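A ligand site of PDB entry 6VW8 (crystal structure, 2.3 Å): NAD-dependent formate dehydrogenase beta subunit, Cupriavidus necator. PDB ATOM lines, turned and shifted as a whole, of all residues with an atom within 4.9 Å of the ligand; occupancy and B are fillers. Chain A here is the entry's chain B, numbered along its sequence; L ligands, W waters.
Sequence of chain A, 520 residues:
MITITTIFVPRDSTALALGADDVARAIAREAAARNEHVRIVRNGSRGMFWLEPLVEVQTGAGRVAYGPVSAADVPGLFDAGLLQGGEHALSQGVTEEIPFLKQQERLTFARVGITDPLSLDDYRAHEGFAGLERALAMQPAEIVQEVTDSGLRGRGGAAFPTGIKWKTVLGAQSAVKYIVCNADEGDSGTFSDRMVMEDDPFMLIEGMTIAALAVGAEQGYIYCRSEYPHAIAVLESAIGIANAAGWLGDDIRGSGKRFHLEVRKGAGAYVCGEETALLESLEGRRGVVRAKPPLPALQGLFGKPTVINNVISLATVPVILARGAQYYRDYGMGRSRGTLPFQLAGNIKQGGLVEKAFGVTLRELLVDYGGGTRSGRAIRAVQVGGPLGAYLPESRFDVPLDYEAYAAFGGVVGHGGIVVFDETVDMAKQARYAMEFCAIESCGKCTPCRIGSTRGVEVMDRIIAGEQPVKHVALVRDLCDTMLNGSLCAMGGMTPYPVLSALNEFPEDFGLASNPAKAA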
ATOM      1  N   GLY A 154      19.038  -5.760 -17.566  1.00  0.00           N
ATOM      2  CA  GLY A 154      19.801  -5.690 -16.324  1.00  0.00           C
ATOM      3  C   GLY A 154      19.022  -5.010 -15.221  1.00  0.00           C
ATOM      4  O   GLY A 154      18.797  -3.800 -15.302  1.00  0.00           O
ATOM      5  N   ARG A 155      18.607  -5.760 -14.185  1.00  0.00           N
ATOM      6  CA  ARG A 155      17.731  -5.185 -13.167  1.00  0.00           C
ATOM      7  C   ARG A 155      18.460  -4.330 -12.148  1.00  0.00           C
ATOM      8  O   ARG A 155      17.809  -3.732 -11.282  1.00  0.00           O
ATOM      9  CB  ARG A 155      16.938  -6.281 -12.471  1.00  0.00           C
ATOM     10  CG  ARG A 155      16.202  -7.143 -13.446  1.00  0.00           C
ATOM     11  CD  ARG A 155      15.198  -6.386 -14.293  1.00  0.00           C
ATOM     12  NE  ARG A 155      14.285  -7.335 -14.940  1.00  0.00           N
ATOM     13  CZ  ARG A 155      13.773  -7.192 -16.157  1.00  0.00           C
ATOM     14  NH1 ARG A 155      14.057  -6.115 -16.907  1.00  0.00           N
ATOM     15  NH2 ARG A 155      12.975  -8.143 -16.638  1.00  0.00           N
ATOM     16  N   GLY A 156      19.779  -4.250 -12.245  1.00  0.00           N
ATOM     17  CA  GLY A 156      20.485  -3.220 -11.517  1.00  0.00           C
ATOM     18  C   GLY A 156      20.149  -1.819 -11.964  1.00  0.00           C
ATOM     19  O   GLY A 156      20.502  -0.857 -11.264  1.00  0.00           O
ATOM     20  N   GLY A 157      19.489  -1.653 -13.120  1.00  0.00           N
ATOM     21  CA  GLY A 157      18.906  -0.371 -13.500  1.00  0.00           C
ATOM     22  C   GLY A 157      19.418   0.204 -14.813  1.00  0.00           C
ATOM     23  O   GLY A 157      18.686   0.916 -15.500  1.00  0.00           O
ATOM     24  N   ALA A 158      20.681  -0.095 -15.167  1.00  0.00           N
ATOM     25  CA  ALA A 158      21.129   0.273 -16.509  1.00  0.00           C
ATOM     26  C   ALA A 158      20.446  -0.562 -17.581  1.00  0.00           C
ATOM     27  O   ALA A 158      20.536  -0.216 -18.760  1.00  0.00           O
ATOM     28  CB  ALA A 158      22.656   0.160 -16.634  1.00  0.00           C
ATOM     29  N   PHE A 160      20.824  -3.206 -19.347  1.00  0.00           N
ATOM     30  CA  PHE A 160      21.461  -3.788 -20.525  1.00  0.00           C
ATOM     31  C   PHE A 160      20.868  -5.168 -20.801  1.00  0.00           C
ATOM     32  O   PHE A 160      20.643  -5.955 -19.866  1.00  0.00           O
ATOM     33  CB  PHE A 160      22.964  -3.935 -20.297  1.00  0.00           C
ATOM     34  CG  PHE A 160      23.739  -4.223 -21.538  1.00  0.00           C
ATOM     35  CD1 PHE A 160      24.178  -3.176 -22.365  1.00  0.00           C
ATOM     36  CD2 PHE A 160      24.012  -5.532 -21.917  1.00  0.00           C
ATOM     37  CE1 PHE A 160      24.877  -3.424 -23.542  1.00  0.00           C
ATOM     38  CE2 PHE A 160      24.714  -5.801 -23.089  1.00  0.00           C
ATOM     39  CZ  PHE A 160      25.156  -4.746 -23.904  1.00  0.00           C
ATOM     40  N   LYS A 165      24.844  -9.745 -23.113  1.00  0.00           N
ATOM     41  CA  LYS A 165      25.982  -9.757 -22.188  1.00  0.00           C
ATOM     42  C   LYS A 165      26.526 -11.170 -21.980  1.00  0.00           C
ATOM     43  O   LYS A 165      27.739 -11.390 -21.983  1.00  0.00           O
ATOM     44  CB  LYS A 165      25.569  -9.117 -20.857  1.00  0.00           C
ATOM     45  CG  LYS A 165      26.699  -8.937 -19.871  1.00  0.00           C
ATOM     46  CD  LYS A 165      26.167  -8.836 -18.412  1.00  0.00           C
ATOM     47  CE  LYS A 165      25.482  -7.482 -18.171  1.00  0.00           C
ATOM     48  NZ  LYS A 165      25.528  -7.035 -16.734  1.00  0.00           N
ATOM     49  N   ASN A 182      26.203  -9.179  -8.279  1.00  0.00           N
ATOM     50  CA  ASN A 182      26.242  -7.879  -7.607  1.00  0.00           C
ATOM     51  C   ASN A 182      25.110  -7.826  -6.595  1.00  0.00           C
ATOM     52  O   ASN A 182      23.952  -7.622  -6.954  1.00  0.00           O
ATOM     53  CB  ASN A 182      26.113  -6.753  -8.631  1.00  0.00           C
ATOM     54  CG  ASN A 182      26.341  -5.406  -8.021  1.00  0.00           C
ATOM     55  OD1 ASN A 182      26.205  -5.231  -6.792  1.00  0.00           O
ATOM     56  ND2 ASN A 182      26.721  -4.430  -8.842  1.00  0.00           N
ATOM     57  N   ASP A 184      25.402  -5.622  -4.007  1.00  0.00           N
ATOM     58  CA  ASP A 184      25.712  -4.441  -3.219  1.00  0.00           C
ATOM     59  C   ASP A 184      24.490  -3.628  -2.845  1.00  0.00           C
ATOM     60  O   ASP A 184      24.601  -2.766  -1.959  1.00  0.00           O
ATOM     61  CB  ASP A 184      26.659  -3.506  -3.941  1.00  0.00           C
ATOM     62  CG  ASP A 184      27.393  -2.612  -2.971  1.00  0.00           C
ATOM     63  OD1 ASP A 184      28.252  -3.164  -2.230  1.00  0.00           O
ATOM     64  OD2 ASP A 184      27.090  -1.389  -2.897  1.00  0.00           O
ATOM     65  N   GLU A 185      23.347  -3.893  -3.480  1.00  0.00           N
ATOM     66  CA  GLU A 185      22.085  -3.163  -3.311  1.00  0.00           C
ATOM     67  C   GLU A 185      22.232  -1.892  -2.497  1.00  0.00           C
ATOM     68  O   GLU A 185      21.698  -1.780  -1.377  1.00  0.00           O
ATOM     69  CB  GLU A 185      21.038  -4.071  -2.670  1.00  0.00           C
ATOM     70  CG  GLU A 185      19.620  -3.567  -2.857  1.00  0.00           C
ATOM     71  CD  GLU A 185      18.549  -4.603  -2.509  1.00  0.00           C
ATOM     72  OE1 GLU A 185      18.595  -5.216  -1.392  1.00  0.00           O
ATOM     73  OE2 GLU A 185      17.685  -4.820  -3.384  1.00  0.00           O
ATOM     74  N   GLY A 186      22.950  -0.913  -3.042  1.00  0.00           N
ATOM     75  CA  GLY A 186      23.308   0.259  -2.271  1.00  0.00           C
ATOM     76  C   GLY A 186      22.228   1.300  -2.155  1.00  0.00           C
ATOM     77  O   GLY A 186      22.337   2.199  -1.304  1.00  0.00           O
ATOM     78  N   ASP A 193      16.827  -7.280  -3.621  1.00  0.00           N
ATOM     79  CA  ASP A 193      17.987  -8.180  -3.566  1.00  0.00           C
ATOM     80  C   ASP A 193      18.098  -8.824  -2.177  1.00  0.00           C
ATOM     81  O   ASP A 193      18.272 -10.039  -2.058  1.00  0.00           O
ATOM     82  CB  ASP A 193      19.278  -7.454  -3.914  1.00  0.00           C
ATOM     83  CG  ASP A 193      19.253  -6.803  -5.297  1.00  0.00           C
ATOM     84  OD1 ASP A 193      18.385  -7.169  -6.136  1.00  0.00           O
ATOM     85  OD2 ASP A 193      20.104  -5.920  -5.561  1.00  0.00           O
ATOM     86  N   TYR A 270      29.228   2.681  -1.172  1.00  0.00           N
ATOM     87  CA  TYR A 270      28.159   2.646  -2.182  1.00  0.00           C
ATOM     88  C   TYR A 270      28.720   2.445  -3.594  1.00  0.00           C
ATOM     89  O   TYR A 270      28.161   1.678  -4.394  1.00  0.00           O
ATOM     90  CB  TYR A 270      27.323   3.940  -2.095  1.00  0.00           C
ATOM     91  CG  TYR A 270      26.266   4.111  -3.176  1.00  0.00           C
ATOM     92  CD1 TYR A 270      25.145   3.296  -3.197  1.00  0.00           C
ATOM     93  CD2 TYR A 270      26.404   5.073  -4.168  1.00  0.00           C
ATOM     94  CE1 TYR A 270      24.184   3.436  -4.176  1.00  0.00           C
ATOM     95  CE2 TYR A 270      25.438   5.236  -5.162  1.00  0.00           C
ATOM     96  CZ  TYR A 270      24.326   4.406  -5.157  1.00  0.00           C
ATOM     97  OH  TYR A 270      23.367   4.514  -6.132  1.00  0.00           O
ATOM     98  N   VAL A 271      29.866   3.068  -3.916  1.00  0.00           N
ATOM     99  CA  VAL A 271      30.385   2.991  -5.281  1.00  0.00           C
ATOM    100  C   VAL A 271      30.852   1.585  -5.655  1.00  0.00           C
ATOM    101  O   VAL A 271      31.041   1.303  -6.858  1.00  0.00           O
ATOM    102  CB  VAL A 271      31.484   4.059  -5.471  1.00  0.00           C
ATOM    103  CG1 VAL A 271      32.224   3.947  -6.839  1.00  0.00           C
ATOM    104  CG2 VAL A 271      30.830   5.403  -5.401  1.00  0.00           C
ATOM    105  N   GLY A 273      28.913  -0.799  -5.618  1.00  0.00           N
ATOM    106  CA  GLY A 273      27.849  -1.286  -6.491  1.00  0.00           C
ATOM    107  C   GLY A 273      28.158  -1.114  -7.965  1.00  0.00           C
ATOM    108  O   GLY A 273      27.567  -1.813  -8.795  1.00  0.00           O
ATOM    109  N   GLU A 274      29.065  -0.196  -8.315  1.00  0.00           N
ATOM    110  CA  GLU A 274      29.452  -0.011  -9.705  1.00  0.00           C
ATOM    111  C   GLU A 274      30.277  -1.199 -10.152  1.00  0.00           C
ATOM    112  O   GLU A 274      31.239  -1.564  -9.494  1.00  0.00           O
ATOM    113  CB  GLU A 274      30.255   1.283  -9.875  1.00  0.00           C
ATOM    114  CG  GLU A 274      30.325   1.788 -11.306  1.00  0.00           C
ATOM    115  CD  GLU A 274      31.376   1.105 -12.145  1.00  0.00           C
ATOM    116  OE1 GLU A 274      32.401   0.626 -11.603  1.00  0.00           O
ATOM    117  OE2 GLU A 274      31.182   1.049 -13.374  1.00  0.00           O
ATOM    118  N   GLU A 275      29.933  -1.771 -11.314  1.00  0.00           N
ATOM    119  CA  GLU A 275      30.420  -3.108 -11.681  1.00  0.00           C
ATOM    120  C   GLU A 275      31.952  -3.218 -11.658  1.00  0.00           C
ATOM    121  O   GLU A 275      32.486  -4.253 -11.236  1.00  0.00           O
ATOM    122  CB  GLU A 275      29.859  -3.515 -13.052  1.00  0.00           C
ATOM    123  CG  GLU A 275      30.192  -2.575 -14.228  1.00  0.00           C
ATOM    124  CD  GLU A 275      29.916  -3.205 -15.583  1.00  0.00           C
ATOM    125  OE1 GLU A 275      28.999  -4.033 -15.725  1.00  0.00           O
ATOM    126  OE2 GLU A 275      30.643  -2.873 -16.541  1.00  0.00           O
ATOM    127  N   ILE A 308      28.710 -10.148 -14.951  1.00  0.00           N
ATOM    128  CA  ILE A 308      28.354  -9.356 -13.790  1.00  0.00           C
ATOM    129  C   ILE A 308      26.866  -9.051 -13.886  1.00  0.00           C
ATOM    130  O   ILE A 308      26.447  -8.309 -14.774  1.00  0.00           O
ATOM    131  CB  ILE A 308      29.150  -8.052 -13.679  1.00  0.00           C
ATOM    132  CG1 ILE A 308      30.635  -8.329 -13.790  1.00  0.00           C
ATOM    133  CG2 ILE A 308      28.815  -7.341 -12.359  1.00  0.00           C
ATOM    134  CD1 ILE A 308      31.472  -7.053 -13.921  1.00  0.00           C
ATOM    135  N   ASN A 309      26.075  -9.590 -12.957  1.00  0.00           N
ATOM    136  CA  ASN A 309      24.649  -9.303 -12.959  1.00  0.00           C
ATOM    137  C   ASN A 309      24.171  -9.044 -11.541  1.00  0.00           C
ATOM    138  O   ASN A 309      24.725  -9.540 -10.564  1.00  0.00           O
ATOM    139  CB  ASN A 309      23.803 -10.452 -13.580  1.00  0.00           C
ATOM    140  CG  ASN A 309      23.774 -10.424 -15.113  1.00  0.00           C
ATOM    141  OD1 ASN A 309      24.259 -11.351 -15.775  1.00  0.00           O
ATOM    142  ND2 ASN A 309      23.172  -9.371 -15.680  1.00  0.00           N
ATOM    143  N   ASN A 310      23.095  -8.279 -11.479  1.00  0.00           N
ATOM    144  CA  ASN A 310      22.394  -7.947 -10.263  1.00  0.00           C
ATOM    145  C   ASN A 310      21.626  -9.174  -9.740  1.00  0.00           C
ATOM    146  O   ASN A 310      21.312 -10.110 -10.479  1.00  0.00           O
ATOM    147  CB  ASN A 310      21.456  -6.779 -10.584  1.00  0.00           C
ATOM    148  CG  ASN A 310      20.394  -6.571  -9.533  1.00  0.00           C
ATOM    149  OD1 ASN A 310      19.283  -7.067  -9.689  1.00  0.00           O
ATOM    150  ND2 ASN A 310      20.724  -5.829  -8.463  1.00  0.00           N
ATOM    151  N   VAL A 311      21.333  -9.164  -8.428  1.00  0.00           N
ATOM    152  CA  VAL A 311      20.661 -10.303  -7.790  1.00  0.00           C
ATOM    153  C   VAL A 311      19.377 -10.670  -8.517  1.00  0.00           C
ATOM    154  O   VAL A 311      19.130 -11.837  -8.831  1.00  0.00           O
ATOM    155  CB  VAL A 311      20.379  -9.999  -6.308  1.00  0.00           C
ATOM    156  CG1 VAL A 311      19.351 -10.993  -5.753  1.00  0.00           C
ATOM    157  CG2 VAL A 311      21.662 -10.024  -5.496  1.00  0.00           C
ATOM    158  N   SER A 313      18.379  -9.866 -11.619  1.00  0.00           N
ATOM    159  CA  SER A 313      18.630 -10.400 -12.953  1.00  0.00           C
ATOM    160  C   SER A 313      18.987 -11.885 -12.880  1.00  0.00           C
ATOM    161  O   SER A 313      18.420 -12.704 -13.613  1.00  0.00           O
ATOM    162  CB  SER A 313      19.762  -9.666 -13.708  1.00  0.00           C
ATOM    163  OG  SER A 313      19.766  -8.264 -13.539  1.00  0.00           O
ATOM    164  N   LEU A 388      20.331   8.156  -6.986  1.00  0.00           N
ATOM    165  CA  LEU A 388      20.642   8.781  -8.269  1.00  0.00           C
ATOM    166  C   LEU A 388      19.394   9.025  -9.114  1.00  0.00           C
ATOM    167  O   LEU A 388      19.502   9.590 -10.215  1.00  0.00           O
ATOM    168  CB  LEU A 388      21.653   7.925  -9.053  1.00  0.00           C
ATOM    169  CG  LEU A 388      22.959   7.508  -8.376  1.00  0.00           C
ATOM    170  CD1 LEU A 388      23.825   6.711  -9.349  1.00  0.00           C
ATOM    171  CD2 LEU A 388      23.754   8.715  -7.845  1.00  0.00           C
ATOM    172  N   CYS A 489      31.388   7.749 -13.946  1.00  0.00           N
ATOM    173  CA  CYS A 489      30.317   6.781 -13.692  1.00  0.00           C
ATOM    174  C   CYS A 489      29.097   7.523 -13.150  1.00  0.00           C
ATOM    175  O   CYS A 489      29.172   8.688 -12.749  1.00  0.00           O
ATOM    176  CB  CYS A 489      30.798   5.662 -12.746  1.00  0.00           C
ATOM    177  SG  CYS A 489      30.569   5.901 -10.974  1.00  0.00           S
ATOM    178  N   ALA A 490      27.975   6.806 -13.099  1.00  0.00           N
ATOM    179  CA  ALA A 490      26.727   7.448 -12.728  1.00  0.00           C
ATOM    180  C   ALA A 490      26.705   7.979 -11.296  1.00  0.00           C
ATOM    181  O   ALA A 490      25.779   8.720 -10.956  1.00  0.00           O
ATOM    182  CB  ALA A 490      25.563   6.475 -12.936  1.00  0.00           C
ATOM    183  N   MET A 491      27.673   7.650 -10.452  1.00  0.00           N
ATOM    184  CA  MET A 491      27.686   8.282  -9.130  1.00  0.00           C
ATOM    185  C   MET A 491      27.865   9.787  -9.263  1.00  0.00           C
ATOM    186  O   MET A 491      27.074  10.576  -8.754  1.00  0.00           O
ATOM    187  CB  MET A 491      28.780   7.689  -8.248  1.00  0.00           C
ATOM    188  CG  MET A 491      29.084   8.524  -7.013  1.00  0.00           C
ATOM    189  SD  MET A 491      27.998   8.040  -5.681  1.00  0.00           S
ATOM    190  CE  MET A 491      26.640   9.207  -5.836  1.00  0.00           C
HETATM  191  N1  LIG L   1      24.026  -2.723  -9.726  1.00  0.00           N
HETATM  192  C1  LIG L   1      23.461  -3.671  -8.755  1.00  0.00           C
HETATM  193  O1  LIG L   1      23.004  -4.701  -9.125  1.00  0.00           O
HETATM  194  N2  LIG L   1      23.431  -3.336  -7.305  1.00  0.00           N
HETATM  195  C2  LIG L   1      23.979  -2.068  -6.855  1.00  0.00           C
HETATM  196  O2  LIG L   1      23.999  -1.769  -5.716  1.00  0.00           O
HETATM  197  C3  LIG L   1      24.572  -1.123  -7.867  1.00  0.00           C
HETATM  198  N3  LIG L   1      25.123   0.133  -7.409  1.00  0.00           N
HETATM  199  C4  LIG L   1      25.719   1.090  -8.378  1.00  0.00           C
HETATM  200  C5  LIG L   1      26.264   2.278  -7.878  1.00  0.00           C
HETATM  201  C6  LIG L   1      26.825   3.211  -8.764  1.00  0.00           C
HETATM  202  C7  LIG L   1      27.331   4.423  -7.949  1.00  0.00           C
HETATM  203  C8  LIG L   1      26.859   2.957 -10.157  1.00  0.00           C
HETATM  204  C9  LIG L   1      27.445   3.923 -11.227  1.00  0.00           C
HETATM  205  C10 LIG L   1      26.300   1.736 -10.638  1.00  0.00           C
HETATM  206  C11 LIG L   1      25.730   0.793  -9.750  1.00  0.00           C
HETATM  207  N4  LIG L   1      25.141  -0.514 -10.206  1.00  0.00           N
HETATM  208  C12 LIG L   1      24.567  -1.447  -9.261  1.00  0.00           C
HETATM  209  C13 LIG L   1      25.089  -0.934 -11.624  1.00  0.00           C
HETATM  210  C14 LIG L   1      26.219  -1.892 -11.975  1.00  0.00           C
HETATM  211  O3  LIG L   1      27.281  -1.058 -12.273  1.00  0.00           O
HETATM  212  C15 LIG L   1      25.772  -2.696 -13.191  1.00  0.00           C
HETATM  213  O4  LIG L   1      25.016  -1.883 -14.043  1.00  0.00           O
HETATM  214  C16 LIG L   1      24.870  -3.869 -12.785  1.00  0.00           C
HETATM  215  O5  LIG L   1      25.304  -4.492 -11.602  1.00  0.00           O
HETATM  216  C17 LIG L   1      24.899  -4.858 -13.943  1.00  0.00           C
HETATM  217  O6  LIG L   1      24.085  -5.972 -13.586  1.00  0.00           O
HETATM  218  P1  LIG L   1      22.664  -6.082 -14.422  1.00  0.00           P
HETATM  219  O7  LIG L   1      21.957  -7.394 -14.115  1.00  0.00           O
HETATM  220  O8  LIG L   1      23.006  -5.982 -15.899  1.00  0.00           O
HETATM  221  O9  LIG L   1      21.812  -4.890 -13.998  1.00  0.00           O
HETATM  222  O   HOH W   1      22.621  -5.392  -5.699  1.00  0.00           O
HETATM  223  O   HOH W   2      22.604  -3.680 -17.093  1.00  0.00           O
HETATM  224  O   HOH W   3      28.003   4.270 -14.466  1.00  0.00           O
HETATM  225  O   HOH W   4      22.071  -7.507 -17.950  1.00  0.00           O
HETATM  226  O   HOH W   5      26.832   1.132 -14.401  1.00  0.00           O
HETATM  227  O   HOH W   6      25.713   0.177  -4.613  1.00  0.00           O
HETATM  228  O   HOH W   7      22.354  -2.348 -14.562  1.00  0.00           O
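ND2 of Asn 310 sits at hydrogen-bond distance from OD2 of Asp 193, at 3.0 Å. ND2 of Asn 309 lies close to NZ of Lys 165, 3.5 Å away. The backbone carbonyl oxygen (O) of Asn 309 sits at hydrogen-bond distance from the backbone NH (N) of Asn 182 (2.7 Å). The backbone NH (N) of Gly 154 lies within hydrogen-bond range of the backbone carbonyl oxygen (O) of Phe 160 (2.8 Å). The side-chain amide nitrogen of Asn 182 is in hydrogen-bond range of the backbone carbonyl oxygen of Gly 273, at 2.8 Å. OD2 of Asp 184 lies within hydrogen-bond range of N of Gly 273 (3.3 Å). OD1 of Asn 182 is in hydrogen-bond range of N of Asp 184, at 2.9 Å. The backbone NH (N) of Asp 193 sits at hydrogen-bond distance from the side-chain carboxylate (OE2) of Glu 185.
The side-chain hydroxyl (OG) of Ser 313 lies within hydrogen-bond range of an oxygen (O7) of the ligand (2.4 Å). O7 of the ligand lies within hydrogen-bond range of N of Asn 310 (3.0 Å). An oxygen (O1) of the ligand lies within hydrogen-bond range of the side-chain amide nitrogen (ND2) of Asn 310, 2.6 Å away. The backbone NH of Gly 156 lies within hydrogen-bond range of an oxygen (O9) of the ligand (2.8 Å). An oxygen (O7) of the ligand lies within hydrogen-bond range of the side-chain amide nitrogen of Asn 309, at 2.8 Å. NZ of Lys 165 lies within salt-bridge range of O8 of the ligand (2.9 Å). N of Glu 275 is in hydrogen-bond range of O3 of the ligand, 2.9 Å away. The backbone NH (N) of Gly 186 sits at hydrogen-bond distance from an oxygen (O2) of the ligand, 3.0 Å away. The side-chain amide nitrogen (ND2) of Asn 182 is in hydrogen-bond range of an oxygen (O5) of the ligand (3.1 Å). An oxygen (O2) of the ligand lies within hydrogen-bond range of the backbone NH of Glu 185 (3.2 Å). N of Arg 155 is in hydrogen-bond range of O9 of the ligand, 3.3 Å away.
An oxygen (O9) of the ligand sits close to the backbone carbonyl oxygen of Gly 154, at 3.5 Å. O of Gly 273 lies close to N4 of the ligand, at 3.1 Å. Merely in contact with the ligand: Asp 184 (3.5 Å), Tyr 270 (3.5 Å), Ala 490 (3.5 Å), Glu 274 (3.5 Å), Ile 308 (3.5 Å), Met 491 (3.6 Å) and Cys 489 (3.7 Å). Hydrophobic or aromatic side chains within 4 Å of the ligand: Tyr 270, Ala 490 and Met 491. The nearest printed residue that does not touch the ligand is Ala 158 (4.1 Å).
Water W2 lies within hydrogen-bond range of O8 of the ligand (2.6 Å) and N of Phe 160 (2.9 Å). Water W7 lies within hydrogen-bond range of O9 of the ligand, N of Ala 158 and N of Gly 157. Water W4 lies within hydrogen-bond range of an oxygen (O8) of the ligand (2.7 Å), the backbone carbonyl oxygen (O) of Phe 160 (2.8 Å) and the side-chain amide nitrogen (ND2) of Asn 309 (3.1 Å).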
